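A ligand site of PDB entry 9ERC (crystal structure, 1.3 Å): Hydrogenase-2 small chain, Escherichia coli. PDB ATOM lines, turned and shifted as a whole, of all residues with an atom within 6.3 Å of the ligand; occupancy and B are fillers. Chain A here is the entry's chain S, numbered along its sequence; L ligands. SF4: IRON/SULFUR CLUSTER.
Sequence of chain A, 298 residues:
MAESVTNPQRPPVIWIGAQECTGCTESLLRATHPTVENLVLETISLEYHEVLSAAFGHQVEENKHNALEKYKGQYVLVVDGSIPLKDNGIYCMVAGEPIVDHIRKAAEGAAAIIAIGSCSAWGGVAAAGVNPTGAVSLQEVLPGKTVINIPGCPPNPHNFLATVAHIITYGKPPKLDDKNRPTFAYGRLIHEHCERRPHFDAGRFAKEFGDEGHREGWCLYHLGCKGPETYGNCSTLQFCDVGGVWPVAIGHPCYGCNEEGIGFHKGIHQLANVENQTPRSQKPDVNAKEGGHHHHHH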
ATOM      1  N   ILE A 190      -3.203  17.174   3.393  1.00  0.00           N
ATOM      2  CA  ILE A 190      -2.115  17.602   2.513  1.00  0.00           C
ATOM      3  C   ILE A 190      -1.182  16.425   2.211  1.00  0.00           C
ATOM      4  O   ILE A 190      -0.820  16.189   1.065  1.00  0.00           O
ATOM      5  CB  ILE A 190      -1.418  18.842   3.118  1.00  0.00           C
ATOM      6  CG1 ILE A 190      -2.356  20.060   3.058  1.00  0.00           C
ATOM      7  CG2 ILE A 190      -0.106  19.097   2.421  1.00  0.00           C
ATOM      8  CD1 ILE A 190      -1.858  21.263   3.854  1.00  0.00           C
ATOM      9  N   HIS A 191      -0.836  15.641   3.239  1.00  0.00           N
ATOM     10  CA  HIS A 191       0.071  14.502   3.076  1.00  0.00           C
ATOM     11  C   HIS A 191      -0.523  13.399   2.214  1.00  0.00           C
ATOM     12  O   HIS A 191       0.245  12.569   1.726  1.00  0.00           O
ATOM     13  CB  HIS A 191       0.381  13.950   4.467  1.00  0.00           C
ATOM     14  CG  HIS A 191       1.322  12.813   4.559  1.00  0.00           C
ATOM     15  ND1 HIS A 191       2.688  12.872   4.399  1.00  0.00           N
ATOM     16  CD2 HIS A 191       1.022  11.526   4.902  1.00  0.00           C
ATOM     17  CE1 HIS A 191       3.192  11.674   4.642  1.00  0.00           C
ATOM     18  NE2 HIS A 191       2.211  10.836   4.904  1.00  0.00           N
ATOM     19  N   GLU A 192      -1.862  13.370   2.026  1.00  0.00           N
ATOM     20  CA  GLU A 192      -2.498  12.379   1.181  1.00  0.00           C
ATOM     21  C   GLU A 192      -2.616  12.898  -0.249  1.00  0.00           C
ATOM     22  O   GLU A 192      -3.280  12.261  -1.080  1.00  0.00           O
ATOM     23  CB  GLU A 192      -3.836  11.926   1.746  1.00  0.00           C
ATOM     24  CG  GLU A 192      -3.662  11.104   3.030  1.00  0.00           C
ATOM     25  CD  GLU A 192      -2.769   9.872   2.875  1.00  0.00           C
ATOM     26  OE1 GLU A 192      -1.819   9.694   3.682  1.00  0.00           O
ATOM     27  OE2 GLU A 192      -2.999   9.078   1.945  1.00  0.00           O
ATOM     28  N   CYS A 194       0.492  15.016  -1.496  1.00  0.00           N
ATOM     29  CA  CYS A 194       1.723  15.791  -1.505  1.00  0.00           C
ATOM     30  C   CYS A 194       2.739  15.152  -2.438  1.00  0.00           C
ATOM     31  O   CYS A 194       3.014  13.924  -2.338  1.00  0.00           O
ATOM     32  CB  CYS A 194       2.314  15.911  -0.103  1.00  0.00           C
ATOM     33  SG  CYS A 194       3.917  16.758  -0.066  1.00  0.00           S
ATOM     34  N   GLU A 195       3.353  15.976  -3.305  1.00  0.00           N
ATOM     35  CA  GLU A 195       4.318  15.515  -4.286  1.00  0.00           C
ATOM     36  C   GLU A 195       5.599  14.993  -3.657  1.00  0.00           C
ATOM     37  O   GLU A 195       6.428  14.401  -4.366  1.00  0.00           O
ATOM     38  CB  GLU A 195       4.592  16.591  -5.337  1.00  0.00           C
ATOM     39  CG  GLU A 195       5.316  17.829  -4.833  1.00  0.00           C
ATOM     40  CD  GLU A 195       4.486  18.942  -4.210  1.00  0.00           C
ATOM     41  OE1 GLU A 195       3.275  18.699  -3.849  1.00  0.00           O
ATOM     42  OE2 GLU A 195       5.055  20.058  -4.100  1.00  0.00           O
ATOM     43  N   ARG A 196       5.811  15.202  -2.330  1.00  0.00           N
ATOM     44  CA  ARG A 196       7.019  14.698  -1.714  1.00  0.00           C
ATOM     45  C   ARG A 196       6.755  13.361  -1.012  1.00  0.00           C
ATOM     46  O   ARG A 196       7.674  12.781  -0.447  1.00  0.00           O
ATOM     47  CB  ARG A 196       7.621  15.722  -0.753  1.00  0.00           C
ATOM     48  CG  ARG A 196       7.972  16.991  -1.505  1.00  0.00           C
ATOM     49  CD  ARG A 196       8.860  17.914  -0.727  1.00  0.00           C
ATOM     50  NE  ARG A 196       9.206  19.029  -1.586  1.00  0.00           N
ATOM     51  CZ  ARG A 196      10.183  19.884  -1.359  1.00  0.00           C
ATOM     52  NH1 ARG A 196      10.936  19.741  -0.287  1.00  0.00           N
ATOM     53  NH2 ARG A 196      10.395  20.885  -2.195  1.00  0.00           N
ATOM     54  N   ARG A 197       5.544  12.850  -1.138  1.00  0.00           N
ATOM     55  CA  ARG A 197       5.232  11.546  -0.561  1.00  0.00           C
ATOM     56  C   ARG A 197       6.206  10.466  -0.999  1.00  0.00           C
ATOM     57  O   ARG A 197       6.546   9.575  -0.191  1.00  0.00           O
ATOM     58  CB  ARG A 197       3.800  11.137  -0.887  1.00  0.00           C
ATOM     59  CG  ARG A 197       3.403   9.821  -0.234  1.00  0.00           C
ATOM     60  CD  ARG A 197       3.497   9.838   1.287  1.00  0.00           C
ATOM     61  NE  ARG A 197       2.935   8.623   1.836  1.00  0.00           N
ATOM     62  CZ  ARG A 197       1.643   8.424   2.060  1.00  0.00           C
ATOM     63  NH1 ARG A 197       0.785   9.418   2.191  1.00  0.00           N
ATOM     64  NH2 ARG A 197       1.219   7.186   2.266  1.00  0.00           N
ATOM     65  N   PRO A 198       6.668  10.395  -2.266  1.00  0.00           N
ATOM     66  CA  PRO A 198       7.641   9.344  -2.603  1.00  0.00           C
ATOM     67  C   PRO A 198       8.894   9.375  -1.728  1.00  0.00           C
ATOM     68  O   PRO A 198       9.492   8.314  -1.423  1.00  0.00           O
ATOM     69  CB  PRO A 198       8.001   9.663  -4.060  1.00  0.00           C
ATOM     70  CG  PRO A 198       6.814  10.410  -4.586  1.00  0.00           C
ATOM     71  CD  PRO A 198       6.328  11.246  -3.430  1.00  0.00           C
ATOM     72  N   PHE A 200       9.091  10.682   1.404  1.00  0.00           N
ATOM     73  CA  PHE A 200       8.628  10.160   2.683  1.00  0.00           C
ATOM     74  C   PHE A 200       8.700   8.635   2.669  1.00  0.00           C
ATOM     75  O   PHE A 200       9.207   8.008   3.605  1.00  0.00           O
ATOM     76  CB  PHE A 200       7.213  10.660   2.938  1.00  0.00           C
ATOM     77  CG  PHE A 200       6.598  10.177   4.236  1.00  0.00           C
ATOM     78  CD1 PHE A 200       5.912   8.977   4.300  1.00  0.00           C
ATOM     79  CD2 PHE A 200       6.674  10.958   5.384  1.00  0.00           C
ATOM     80  CE1 PHE A 200       5.324   8.554   5.483  1.00  0.00           C
ATOM     81  CE2 PHE A 200       6.100  10.515   6.570  1.00  0.00           C
ATOM     82  CZ  PHE A 200       5.424   9.320   6.621  1.00  0.00           C
ATOM     83  N   PHE A 205      14.737  12.220   3.612  1.00  0.00           N
ATOM     84  CA  PHE A 205      14.271  13.330   4.445  1.00  0.00           C
ATOM     85  C   PHE A 205      15.336  14.416   4.545  1.00  0.00           C
ATOM     86  O   PHE A 205      16.511  14.163   4.761  1.00  0.00           O
ATOM     87  CB  PHE A 205      13.967  12.839   5.865  1.00  0.00           C
ATOM     88  CG  PHE A 205      12.862  11.836   5.993  1.00  0.00           C
ATOM     89  CD1 PHE A 205      11.538  12.183   5.752  1.00  0.00           C
ATOM     90  CD2 PHE A 205      13.118  10.536   6.432  1.00  0.00           C
ATOM     91  CE1 PHE A 205      10.515  11.276   5.917  1.00  0.00           C
ATOM     92  CE2 PHE A 205      12.083   9.641   6.600  1.00  0.00           C
ATOM     93  CZ  PHE A 205      10.790   9.992   6.338  1.00  0.00           C
ATOM     94  N   TRP A 218      13.607  16.867  -0.945  1.00  0.00           N
ATOM     95  CA  TRP A 218      13.115  15.708  -0.215  1.00  0.00           C
ATOM     96  C   TRP A 218      12.012  16.089   0.767  1.00  0.00           C
ATOM     97  O   TRP A 218      11.708  17.259   0.971  1.00  0.00           O
ATOM     98  CB  TRP A 218      14.294  15.041   0.509  1.00  0.00           C
ATOM     99  CG  TRP A 218      15.218  14.295  -0.420  1.00  0.00           C
ATOM    100  CD1 TRP A 218      15.137  14.208  -1.775  1.00  0.00           C
ATOM    101  CD2 TRP A 218      16.375  13.536  -0.036  1.00  0.00           C
ATOM    102  NE1 TRP A 218      16.185  13.468  -2.281  1.00  0.00           N
ATOM    103  CE2 TRP A 218      16.947  13.013  -1.228  1.00  0.00           C
ATOM    104  CE3 TRP A 218      16.974  13.241   1.187  1.00  0.00           C
ATOM    105  CZ2 TRP A 218      18.069  12.189  -1.214  1.00  0.00           C
ATOM    106  CZ3 TRP A 218      18.075  12.418   1.208  1.00  0.00           C
ATOM    107  CH2 TRP A 218      18.624  11.913   0.012  1.00  0.00           C
ATOM    108  N   CYS A 219      11.408  15.079   1.382  1.00  0.00           N
ATOM    109  CA  CYS A 219      10.303  15.274   2.300  1.00  0.00           C
ATOM    110  C   CYS A 219      10.770  16.058   3.530  1.00  0.00           C
ATOM    111  O   CYS A 219      11.909  15.921   3.988  1.00  0.00           O
ATOM    112  CB  CYS A 219       9.696  13.930   2.660  1.00  0.00           C
ATOM    113  SG  CYS A 219       8.561  13.900   4.070  1.00  0.00           S
ATOM    114  N   LEU A 220       9.867  16.890   4.052  1.00  0.00           N
ATOM    115  CA  LEU A 220      10.129  17.775   5.169  1.00  0.00           C
ATOM    116  C   LEU A 220       9.548  17.272   6.486  1.00  0.00           C
ATOM    117  O   LEU A 220       9.466  18.032   7.452  1.00  0.00           O
ATOM    118  CB  LEU A 220       9.567  19.159   4.800  1.00  0.00           C
ATOM    119  CG  LEU A 220      10.043  19.741   3.463  1.00  0.00           C
ATOM    120  CD1 LEU A 220       9.554  21.200   3.322  1.00  0.00           C
ATOM    121  CD2 LEU A 220      11.541  19.681   3.330  1.00  0.00           C
ATOM    122  N   TYR A 221       9.140  16.000   6.562  1.00  0.00           N
ATOM    123  CA  TYR A 221       8.536  15.439   7.756  1.00  0.00           C
ATOM    124  C   TYR A 221       9.417  15.699   8.994  1.00  0.00           C
ATOM    125  O   TYR A 221       8.914  16.181  10.033  1.00  0.00           O
ATOM    126  CB  TYR A 221       8.258  13.935   7.594  1.00  0.00           C
ATOM    127  CG  TYR A 221       7.695  13.352   8.857  1.00  0.00           C
ATOM    128  CD1 TYR A 221       6.377  13.570   9.211  1.00  0.00           C
ATOM    129  CD2 TYR A 221       8.539  12.724   9.772  1.00  0.00           C
ATOM    130  CE1 TYR A 221       5.848  13.104  10.407  1.00  0.00           C
ATOM    131  CE2 TYR A 221       8.053  12.292  10.990  1.00  0.00           C
ATOM    132  CZ  TYR A 221       6.708  12.505  11.306  1.00  0.00           C
ATOM    133  OH  TYR A 221       6.208  12.096  12.508  1.00  0.00           O
ATOM    134  N   HIS A 222      10.731  15.423   8.867  1.00  0.00           N
ATOM    135  CA  HIS A 222      11.642  15.555  10.011  1.00  0.00           C
ATOM    136  C   HIS A 222      12.005  17.002  10.307  1.00  0.00           C
ATOM    137  O   HIS A 222      12.726  17.230  11.273  1.00  0.00           O
ATOM    138  CB  HIS A 222      12.877  14.609   9.906  1.00  0.00           C
ATOM    139  CG  HIS A 222      12.481  13.225  10.268  1.00  0.00           C
ATOM    140  ND1 HIS A 222      12.279  12.825  11.566  1.00  0.00           N
ATOM    141  CD2 HIS A 222      12.226  12.136   9.482  1.00  0.00           C
ATOM    142  CE1 HIS A 222      11.814  11.564  11.541  1.00  0.00           C
ATOM    143  NE2 HIS A 222      11.805  11.116  10.280  1.00  0.00           N
ATOM    144  N   CYS A 225       6.995  18.937   9.326  1.00  0.00           N
ATOM    145  CA  CYS A 225       5.860  19.096   8.437  1.00  0.00           C
ATOM    146  C   CYS A 225       4.573  18.567   9.059  1.00  0.00           C
ATOM    147  O   CYS A 225       4.487  17.415   9.487  1.00  0.00           O
ATOM    148  CB  CYS A 225       6.138  18.452   7.089  1.00  0.00           C
ATOM    149  SG  CYS A 225       4.838  18.838   5.886  1.00  0.00           S
ATOM    150  N   LYS A 226       3.530  19.409   9.036  1.00  0.00           N
ATOM    151  CA  LYS A 226       2.234  19.063   9.590  1.00  0.00           C
ATOM    152  C   LYS A 226       1.264  18.561   8.535  1.00  0.00           C
ATOM    153  O   LYS A 226       0.083  18.354   8.796  1.00  0.00           O
ATOM    154  CB  LYS A 226       1.658  20.239  10.363  1.00  0.00           C
ATOM    155  CG  LYS A 226       2.514  20.715  11.532  1.00  0.00           C
ATOM    156  CD  LYS A 226       3.064  19.600  12.410  1.00  0.00           C
ATOM    157  CE  LYS A 226       3.738  20.151  13.643  1.00  0.00           C
ATOM    158  NZ  LYS A 226       4.850  21.071  13.330  1.00  0.00           N
ATOM    159  N   GLY A 227       1.757  18.362   7.306  1.00  0.00           N
ATOM    160  CA  GLY A 227       0.912  17.850   6.244  1.00  0.00           C
ATOM    161  C   GLY A 227       0.141  16.597   6.671  1.00  0.00           C
ATOM    162  O   GLY A 227      -1.020  16.395   6.289  1.00  0.00           O
ATOM    163  N   PRO A 228       0.764  15.675   7.443  1.00  0.00           N
ATOM    164  CA  PRO A 228       0.052  14.481   7.891  1.00  0.00           C
ATOM    165  C   PRO A 228      -1.194  14.690   8.752  1.00  0.00           C
ATOM    166  O   PRO A 228      -2.020  13.785   8.857  1.00  0.00           O
ATOM    167  CB  PRO A 228       1.151  13.662   8.565  1.00  0.00           C
ATOM    168  CG  PRO A 228       2.449  14.136   7.932  1.00  0.00           C
ATOM    169  CD  PRO A 228       2.214  15.628   7.710  1.00  0.00           C
ATOM    170  N   TRP A 246       3.952  26.808  -2.821  1.00  0.00           N
ATOM    171  CA  TRP A 246       3.343  26.568  -1.518  1.00  0.00           C
ATOM    172  C   TRP A 246       4.483  26.345  -0.529  1.00  0.00           C
ATOM    173  O   TRP A 246       5.649  26.198  -0.942  1.00  0.00           O
ATOM    174  CB  TRP A 246       2.337  25.419  -1.544  1.00  0.00           C
ATOM    175  CG  TRP A 246       2.827  24.010  -1.733  1.00  0.00           C
ATOM    176  CD1 TRP A 246       3.393  23.440  -2.849  1.00  0.00           C
ATOM    177  CD2 TRP A 246       2.730  22.944  -0.764  1.00  0.00           C
ATOM    178  NE1 TRP A 246       3.590  22.099  -2.645  1.00  0.00           N
ATOM    179  CE2 TRP A 246       3.224  21.768  -1.372  1.00  0.00           C
ATOM    180  CE3 TRP A 246       2.236  22.853   0.538  1.00  0.00           C
ATOM    181  CZ2 TRP A 246       3.257  20.547  -0.688  1.00  0.00           C
ATOM    182  CZ3 TRP A 246       2.256  21.647   1.211  1.00  0.00           C
ATOM    183  CH2 TRP A 246       2.717  20.490   0.585  1.00  0.00           C
ATOM    184  N   VAL A 248       5.835  23.979   1.370  1.00  0.00           N
ATOM    185  CA  VAL A 248       6.704  22.824   1.210  1.00  0.00           C
ATOM    186  C   VAL A 248       7.501  22.929  -0.083  1.00  0.00           C
ATOM    187  O   VAL A 248       8.702  22.670  -0.085  1.00  0.00           O
ATOM    188  CB  VAL A 248       5.872  21.540   1.252  1.00  0.00           C
ATOM    189  CG1 VAL A 248       6.668  20.355   0.728  1.00  0.00           C
ATOM    190  CG2 VAL A 248       5.402  21.272   2.682  1.00  0.00           C
ATOM    191  N   PRO A 253       8.441  23.283   6.019  1.00  0.00           N
ATOM    192  CA  PRO A 253       7.325  22.415   6.394  1.00  0.00           C
ATOM    193  C   PRO A 253       5.995  23.162   6.511  1.00  0.00           C
ATOM    194  O   PRO A 253       5.957  24.347   6.826  1.00  0.00           O
ATOM    195  CB  PRO A 253       7.735  21.876   7.783  1.00  0.00           C
ATOM    196  CG  PRO A 253       8.773  22.815   8.255  1.00  0.00           C
ATOM    197  CD  PRO A 253       9.510  23.272   7.019  1.00  0.00           C
ATOM    198  N   CYS A 254       4.915  22.435   6.244  1.00  0.00           N
ATOM    199  CA  CYS A 254       3.588  22.853   6.649  1.00  0.00           C
ATOM    200  C   CYS A 254       3.584  23.004   8.176  1.00  0.00           C
ATOM    201  O   CYS A 254       4.184  22.178   8.859  1.00  0.00           O
ATOM    202  CB  CYS A 254       2.517  21.862   6.215  1.00  0.00           C
ATOM    203  SG  CYS A 254       0.840  22.192   6.767  1.00  0.00           S
HETATM  204 FE1  SF4 L   1       6.580  14.915   3.544  1.00  0.00          FE
HETATM  205 FE2  SF4 L   1       4.970  16.979   4.493  1.00  0.00          FE
HETATM  206 FE3  SF4 L   1       3.903  14.519   3.998  1.00  0.00          FE
HETATM  207 FE4  SF4 L   1       4.682  16.108   1.980  1.00  0.00          FE
HETATM  208  S1  SF4 L   1       2.976  16.537   3.502  1.00  0.00           S
HETATM  209  S2  SF4 L   1       5.147  13.854   2.122  1.00  0.00           S
HETATM  210  S3  SF4 L   1       6.552  17.106   2.817  1.00  0.00           S
HETATM  211  S4  SF4 L   1       5.453  15.004   5.598  1.00  0.00           S
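O of Arg 196 sits close to S2 of the ligand, at 3.8 Å.
Merely in contact with the ligand: Tyr 221, Gly 227, Val 248, Phe 200 and Pro 228.
Within 4 Å of the ligand: His 191, Cys 194, Arg 196, Arg 197, Phe 200, Cys 219, Leu 220, Tyr 221, Cys 225, Gly 227, Pro 228 and Val 248.
The guanidinium group (NH1) of Arg 197 sits at hydrogen-bond distance from the backbone carbonyl oxygen (O) of His 191, 3.2 Å away.
The side-chain sulfur of Cys 219 lies close to the backbone NH of Tyr 221 (3.3 Å).
The side-chain sulfur (SG) of Cys 225 sits close to the backbone NH (N) of Gly 227 (3.4 Å).
The backbone NH (N) of Cys 254 lies close to the side-chain sulfur (SG) of Cys 225.
NH1 of Arg 197 lies within salt-bridge range of OE1 of Glu 192, at 3.0 Å.
SG of Cys 194 sits close to N of Arg 196.
The backbone carbonyl oxygen (O) of Val 248 sits at hydrogen-bond distance from the guanidinium group (NH2) of Arg 196, 3.2 Å away.
O of Trp 218 sits at hydrogen-bond distance from NH1 of Arg 196, at 2.9 Å.
The side-chain sulfur (SG) of Cys 219 is bound to an iron atom (FE1) of the ligand (2.3 Å).
N of Leu 220 lies close to S3 of the ligand (3.5 Å).
S2 of the ligand sits close to N of Arg 197 (3.4 Å).
SG of Cys 225 is bound to FE2 of the ligand (2.3 Å).
An iron atom (FE3) of the ligand is bound by a ring nitrogen (ND1) of His 191, 2.1 Å away.
An iron atom (FE4) of the ligand is bound by the side-chain sulfur of Cys 194.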
